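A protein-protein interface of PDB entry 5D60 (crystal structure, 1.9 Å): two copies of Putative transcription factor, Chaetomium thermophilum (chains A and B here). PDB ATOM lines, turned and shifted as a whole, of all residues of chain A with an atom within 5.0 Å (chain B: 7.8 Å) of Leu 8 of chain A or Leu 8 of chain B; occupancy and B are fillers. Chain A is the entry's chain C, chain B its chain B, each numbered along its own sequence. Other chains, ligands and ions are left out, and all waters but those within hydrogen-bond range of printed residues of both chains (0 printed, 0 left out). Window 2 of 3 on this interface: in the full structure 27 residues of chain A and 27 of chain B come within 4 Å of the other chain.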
ATOM      1  N   GLN A   4       3.912  25.774  -7.759  1.00  0.00           N
ATOM      2  CA  GLN A   4       3.609  24.546  -7.025  1.00  0.00           C
ATOM      3  C   GLN A   4       3.337  23.387  -7.987  1.00  0.00           C
ATOM      4  O   GLN A   4       3.796  22.260  -7.775  1.00  0.00           O
ATOM      5  CB  GLN A   4       2.417  24.786  -6.092  1.00  0.00           C
ATOM      6  CG  GLN A   4       2.128  23.674  -5.088  1.00  0.00           C
ATOM      7  CD  GLN A   4       0.887  23.926  -4.225  1.00  0.00           C
ATOM      8  OE1 GLN A   4       0.109  24.850  -4.478  1.00  0.00           O
ATOM      9  NE2 GLN A   4       0.695  23.080  -3.203  1.00  0.00           N
ATOM     10  N   ILE A   5       2.628  23.693  -9.071  1.00  0.00           N
ATOM     11  CA  ILE A   5       2.218  22.677 -10.053  1.00  0.00           C
ATOM     12  C   ILE A   5       3.365  22.290 -11.015  1.00  0.00           C
ATOM     13  O   ILE A   5       3.449  21.127 -11.426  1.00  0.00           O
ATOM     14  CB  ILE A   5       0.938  23.134 -10.799  1.00  0.00           C
ATOM     15  CG1 ILE A   5      -0.248  23.121  -9.826  1.00  0.00           C
ATOM     16  CG2 ILE A   5       0.621  22.238 -11.976  1.00  0.00           C
ATOM     17  CD1 ILE A   5      -1.483  23.760 -10.370  1.00  0.00           C
ATOM     18  N   ALA A   6       4.267  23.216 -11.318  1.00  0.00           N
ATOM     19  CA  ALA A   6       5.495  22.861 -11.994  1.00  0.00           C
ATOM     20  C   ALA A   6       6.330  21.884 -11.141  1.00  0.00           C
ATOM     21  O   ALA A   6       6.925  20.945 -11.672  1.00  0.00           O
ATOM     22  CB  ALA A   6       6.310  24.105 -12.302  1.00  0.00           C
ATOM     23  N   ALA A   7       6.397  22.097  -9.814  1.00  0.00           N
ATOM     24  CA  ALA A   7       7.163  21.193  -8.957  1.00  0.00           C
ATOM     25  C   ALA A   7       6.510  19.819  -8.846  1.00  0.00           C
ATOM     26  O   ALA A   7       7.208  18.789  -8.733  1.00  0.00           O
ATOM     27  CB  ALA A   7       7.356  21.808  -7.570  1.00  0.00           C
ATOM     28  N   LEU A   8       5.171  19.798  -8.823  1.00  0.00           N
ATOM     29  CA  LEU A   8       4.438  18.529  -8.859  1.00  0.00           C
ATOM     30  C   LEU A   8       4.862  17.741 -10.107  1.00  0.00           C
ATOM     31  O   LEU A   8       5.060  16.510 -10.046  1.00  0.00           O
ATOM     32  CB  LEU A   8       2.901  18.745  -8.772  1.00  0.00           C
ATOM     33  CG  LEU A   8       2.174  18.765  -7.399  1.00  0.00           C
ATOM     34  CD1 LEU A   8       0.671  18.764  -7.631  1.00  0.00           C
ATOM     35  CD2 LEU A   8       2.530  17.618  -6.452  1.00  0.00           C
ATOM     36  N   SER A   9       5.055  18.454 -11.215  1.00  0.00           N
ATOM     37  CA  SER A   9       5.531  17.864 -12.464  1.00  0.00           C
ATOM     38  C   SER A   9       7.025  17.470 -12.500  1.00  0.00           C
ATOM     39  O   SER A   9       7.315  16.385 -12.966  1.00  0.00           O
ATOM     40  CB  SER A   9       5.253  18.802 -13.656  1.00  0.00           C
ATOM     41  OG  SER A   9       3.859  18.940 -13.914  1.00  0.00           O
ATOM     42  N   GLU A  10       7.937  18.353 -12.083  1.00  0.00           N
ATOM     43  CA  GLU A  10       9.434  18.112 -12.127  1.00  0.00           C
ATOM     44  C   GLU A  10       9.876  16.961 -11.149  1.00  0.00           C
ATOM     45  O   GLU A  10      10.864  16.176 -11.363  1.00  0.00           O
ATOM     46  CB  GLU A  10      10.177  19.462 -11.936  1.00  0.00           C
ATOM     47  CG  GLU A  10      11.723  19.511 -12.057  1.00  0.00           C
ATOM     48  CD  GLU A  10      12.446  20.770 -11.465  1.00  0.00           C
ATOM     49  OE1 GLU A  10      13.113  21.565 -12.192  1.00  0.00           O
ATOM     50  OE2 GLU A  10      12.416  20.963 -10.234  1.00  0.00           O
ATOM     51  N   SER A  11       9.083  16.792 -10.106  1.00  0.00           N
ATOM     52  CA  SER A  11       9.204  15.619  -9.265  1.00  0.00           C
ATOM     53  C   SER A  11       8.728  14.378  -9.991  1.00  0.00           C
ATOM     54  O   SER A  11       9.261  13.287  -9.779  1.00  0.00           O
ATOM     55  CB  SER A  11       8.345  15.786  -8.041  1.00  0.00           C
ATOM     56  OG  SER A  11       8.722  14.873  -7.054  1.00  0.00           O
ATOM     57  N   LEU A  12       7.673  14.515 -10.783  1.00  0.00           N
ATOM     58  CA  LEU A  12       7.146  13.361 -11.506  1.00  0.00           C
ATOM     59  C   LEU A  12       8.125  12.893 -12.582  1.00  0.00           C
ATOM     60  O   LEU A  12       8.130  11.710 -12.897  1.00  0.00           O
ATOM     61  CB  LEU A  12       5.755  13.663 -12.061  1.00  0.00           C
ATOM     62  CG  LEU A  12       4.748  12.555 -12.439  1.00  0.00           C
ATOM     63  CD1 LEU A  12       4.189  11.839 -11.213  1.00  0.00           C
ATOM     64  CD2 LEU A  12       3.608  13.182 -13.215  1.00  0.00           C
ATOM     65  N   GLN B   2      -5.582  24.869 -16.219  1.00  0.00           N
ATOM     66  CA  GLN B   2      -6.205  23.598 -16.565  1.00  0.00           C
ATOM     67  C   GLN B   2      -5.181  22.864 -17.431  1.00  0.00           C
ATOM     68  O   GLN B   2      -5.069  21.660 -17.339  1.00  0.00           O
ATOM     69  CB  GLN B   2      -7.516  23.778 -17.326  1.00  0.00           C
ATOM     70  N   GLN B   3      -4.413  23.611 -18.231  1.00  0.00           N
ATOM     71  CA  GLN B   3      -3.359  23.051 -19.080  1.00  0.00           C
ATOM     72  C   GLN B   3      -2.213  22.357 -18.317  1.00  0.00           C
ATOM     73  O   GLN B   3      -1.803  21.238 -18.674  1.00  0.00           O
ATOM     74  CB  GLN B   3      -2.764  24.161 -19.954  1.00  0.00           C
ATOM     75  N   GLN B   4      -1.683  23.033 -17.296  1.00  0.00           N
ATOM     76  CA  GLN B   4      -0.636  22.445 -16.461  1.00  0.00           C
ATOM     77  C   GLN B   4      -1.125  21.146 -15.838  1.00  0.00           C
ATOM     78  O   GLN B   4      -0.393  20.158 -15.791  1.00  0.00           O
ATOM     79  CB  GLN B   4      -0.124  23.422 -15.369  1.00  0.00           C
ATOM     80  CG  GLN B   4       1.292  23.915 -15.639  1.00  0.00           C
ATOM     81  CD  GLN B   4       1.905  24.728 -14.494  1.00  0.00           C
ATOM     82  OE1 GLN B   4       1.354  24.809 -13.398  1.00  0.00           O
ATOM     83  NE2 GLN B   4       3.065  25.335 -14.760  1.00  0.00           N
ATOM     84  N   ILE B   5      -2.379  21.140 -15.420  1.00  0.00           N
ATOM     85  CA  ILE B   5      -2.938  20.002 -14.722  1.00  0.00           C
ATOM     86  C   ILE B   5      -3.320  18.863 -15.679  1.00  0.00           C
ATOM     87  O   ILE B   5      -3.261  17.684 -15.302  1.00  0.00           O
ATOM     88  CB  ILE B   5      -4.117  20.451 -13.824  1.00  0.00           C
ATOM     89  CG1 ILE B   5      -3.582  21.267 -12.661  1.00  0.00           C
ATOM     90  CG2 ILE B   5      -4.896  19.279 -13.258  1.00  0.00           C
ATOM     91  CD1 ILE B   5      -4.644  21.958 -11.856  1.00  0.00           C
ATOM     92  N   ALA B   6      -3.695  19.196 -16.912  1.00  0.00           N
ATOM     93  CA  ALA B   6      -3.859  18.171 -17.945  1.00  0.00           C
ATOM     94  C   ALA B   6      -2.518  17.453 -18.222  1.00  0.00           C
ATOM     95  O   ALA B   6      -2.491  16.231 -18.366  1.00  0.00           O
ATOM     96  CB  ALA B   6      -4.424  18.767 -19.221  1.00  0.00           C
ATOM     97  N   ALA B   7      -1.418  18.203 -18.268  1.00  0.00           N
ATOM     98  CA  ALA B   7      -0.104  17.605 -18.519  1.00  0.00           C
ATOM     99  C   ALA B   7       0.371  16.758 -17.351  1.00  0.00           C
ATOM    100  O   ALA B   7       1.021  15.731 -17.519  1.00  0.00           O
ATOM    101  CB  ALA B   7       0.911  18.683 -18.826  1.00  0.00           C
ATOM    102  N   LEU B   8       0.048  17.184 -16.143  1.00  0.00           N
ATOM    103  CA  LEU B   8       0.305  16.361 -14.988  1.00  0.00           C
ATOM    104  C   LEU B   8      -0.451  15.031 -15.038  1.00  0.00           C
ATOM    105  O   LEU B   8       0.097  13.978 -14.651  1.00  0.00           O
ATOM    106  CB  LEU B   8      -0.036  17.193 -13.787  1.00  0.00           C
ATOM    107  CG  LEU B   8       0.057  16.619 -12.388  1.00  0.00           C
ATOM    108  CD1 LEU B   8       1.403  15.958 -12.170  1.00  0.00           C
ATOM    109  CD2 LEU B   8      -0.184  17.705 -11.347  1.00  0.00           C
ATOM    110  N   SER B   9      -1.682  15.067 -15.539  1.00  0.00           N
ATOM    111  CA  SER B   9      -2.481  13.858 -15.720  1.00  0.00           C
ATOM    112  C   SER B   9      -1.949  12.961 -16.824  1.00  0.00           C
ATOM    113  O   SER B   9      -1.987  11.730 -16.670  1.00  0.00           O
ATOM    114  CB  SER B   9      -3.951  14.191 -16.067  1.00  0.00           C
ATOM    115  OG  SER B   9      -4.665  14.683 -14.963  1.00  0.00           O
ATOM    116  N   GLU B  10      -1.541  13.562 -17.942  1.00  0.00           N
ATOM    117  CA  GLU B  10      -0.860  12.828 -18.993  1.00  0.00           C
ATOM    118  C   GLU B  10       0.324  12.106 -18.367  1.00  0.00           C
ATOM    119  O   GLU B  10       0.600  10.963 -18.685  1.00  0.00           O
ATOM    120  CB  GLU B  10      -0.326  13.769 -20.094  1.00  0.00           C
ATOM    121  CG  GLU B  10      -1.361  14.459 -20.979  1.00  0.00           C
ATOM    122  CD  GLU B  10      -0.792  15.718 -21.629  1.00  0.00           C
ATOM    123  OE1 GLU B  10       0.333  16.110 -21.252  1.00  0.00           O
ATOM    124  OE2 GLU B  10      -1.445  16.320 -22.506  1.00  0.00           O
ATOM    125  N   SER B  11       1.032  12.806 -17.493  1.00  0.00           N
ATOM    126  CA  SER B  11       2.302  12.331 -16.962  1.00  0.00           C
ATOM    127  C   SER B  11       2.118  11.239 -15.916  1.00  0.00           C
ATOM    128  O   SER B  11       2.839  10.230 -15.907  1.00  0.00           O
ATOM    129  CB  SER B  11       3.110  13.548 -16.507  1.00  0.00           C
ATOM    130  OG  SER B  11       3.526  14.214 -17.673  1.00  0.00           O
ATOM    131  N   LEU B  12       1.113  11.382 -15.067  1.00  0.00           N
ATOM    132  CA  LEU B  12       0.858  10.330 -14.063  1.00  0.00           C
ATOM    133  C   LEU B  12       0.299   9.028 -14.704  1.00  0.00           C
ATOM    134  O   LEU B  12       0.520   7.937 -14.173  1.00  0.00           O
ATOM    135  CB  LEU B  12      -0.042  10.867 -12.969  1.00  0.00           C
ATOM    136  CG  LEU B  12      -0.086  10.145 -11.588  1.00  0.00           C
ATOM    137  CD1 LEU B  12      -1.391   9.393 -11.387  1.00  0.00           C
ATOM    138  CD2 LEU B  12       1.057   9.187 -11.343  1.00  0.00           C
ATOM    139  N   GLN B  13      -0.384   9.155 -15.843  1.00  0.00           N
ATOM    140  CA  GLN B  13      -0.841   8.006 -16.623  1.00  0.00           C
ATOM    141  C   GLN B  13       0.317   7.210 -17.175  1.00  0.00           C
ATOM    142  O   GLN B  13       0.300   5.974 -17.142  1.00  0.00           O
ATOM    143  CB  GLN B  13      -1.690   8.453 -17.826  1.00  0.00           C
ATOM    144  CG  GLN B  13      -2.033   7.406 -18.881  1.00  0.00           C
ATOM    145  CD  GLN B  13      -3.251   6.580 -18.498  1.00  0.00           C
ATOM    146  OE1 GLN B  13      -4.391   6.986 -18.778  1.00  0.00           O
ATOM    147  NE2 GLN B  13      -3.030   5.432 -17.839  1.00  0.00           N
ATOM    148  N   ALA B  14       1.303   7.914 -17.708  1.00  0.00           N
ATOM    149  CA  ALA B  14       2.501   7.265 -18.232  1.00  0.00           C
ATOM    150  C   ALA B  14       3.278   6.553 -17.132  1.00  0.00           C
ATOM    151  O   ALA B  14       3.805   5.443 -17.364  1.00  0.00           O
ATOM    152  CB  ALA B  14       3.380   8.281 -18.958  1.00  0.00           C
ATOM    153  N   THR B  15       3.389   7.191 -15.949  1.00  0.00           N
ATOM    154  CA  THR B  15       3.998   6.549 -14.784  1.00  0.00           C
ATOM    155  C   THR B  15       3.290   5.260 -14.398  1.00  0.00           C
ATOM    156  O   THR B  15       3.933   4.219 -14.150  1.00  0.00           O
ATOM    157  CB  THR B  15       3.987   7.543 -13.597  1.00  0.00           C
ATOM    158  OG1 THR B  15       4.769   8.682 -13.948  1.00  0.00           O
ATOM    159  CG2 THR B  15       4.587   6.921 -12.364  1.00  0.00           C
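OG of Ser 11 of chain B is in hydrogen-bond range of O of Ala 7 of chain B (2.9 Å).
O of Ile 5 of chain A lies within hydrogen-bond range of OG of Ser 9 of chain A (3.3 Å).
The backbone carbonyl oxygen of Ile 5 of chain B lies within hydrogen-bond range of the side-chain hydroxyl of Ser 9 of chain B.
The side-chain hydroxyl of Thr 15 of chain B is in hydrogen-bond range of the backbone carbonyl oxygen of Ser 11 of chain B (3.2 Å).
OE1 of Gln 4 of chain B touches CG2 of Ile 5 of chain A, at 3.0 Å.
CD1 of Ile 5 of chain B touches CD1 of Ile 5 of chain A, at 3.9 Å.
Gln 4 of chain B touches Ala 6 of chain A.
Leu 8 of chain B touches Leu 8 of chain A.
CD2 of Leu 12 of chain A touches CD1 of Leu 8 of chain B (3.7 Å).
Ser 11 of chain B touches Leu 12 of chain A.
CD2 of Leu 12 of chain A touches N of Leu 12 of chain B, at 3.6 Å.
Of chain B, only Leu 8 (3.96 Å) comes within 4 Å of Leu 8 of chain A.
Leu 8 of chain B touches just these residues of chain A: Leu 8 (3.96 Å) and Leu 12 (3.7 Å).
No residue of chain B comes within 4 Å of Ala 7 of chain A.
Printed residues of chain B within 4 Å of Leu 12 of chain A: Leu 8 (3.7 Å), Ser 11 (3.3 Å) and Leu 12 (3.6 Å).
Of the printed residues of chain A, Leu 12 of chain B touches Leu 12.
Of the printed residues of chain A, Gln 4 of chain B touches Ile 5 (3.0 Å) and Ala 6 (3.9 Å).
Printed residues of chain B within 4 Å of Ala 6 of chain A: Gln 4 (3.9 Å).
Ser 9 of chain B touches none of the printed residues of chain A.
Thr 15 of chain B touches none of the printed residues of chain A.
The nearest residue of chain A that does not touch Leu 8 of chain B is Ser 9 of chain A (4.2 Å).
Printed residues of chain B that touch a printed residue of chain A: Gln 4, Ile 5, Leu 8, Ser 11 and Leu 12.
Hydrophobic or aromatic side chains of chain B that line the printed part of chain A: Ile 5 and Leu 8.
Among the printed residues, no Asp or Glu carboxylate lies within 4 Å of a Lys or Arg side-chain nitrogen of the other chain.
Ile 5 of chain B touches its own counterpart, Ile 5 of chain A.
Leu 8 of chain A touches its own counterpart, Leu 8 of chain B.
Leu 12 of chain A touches Leu 8 of chain B, but with the chains exchanged Leu 8 of chain A does not touch Leu 12 of chain B (8.1 Å).
Leu 12 of chain B touches its own counterpart, Leu 12 of chain A.
9 positions are printed for both chains.
Of the 7 pairs that touch across the chains among the printed residues, 3 have their exchanged pair printed and touching as well.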
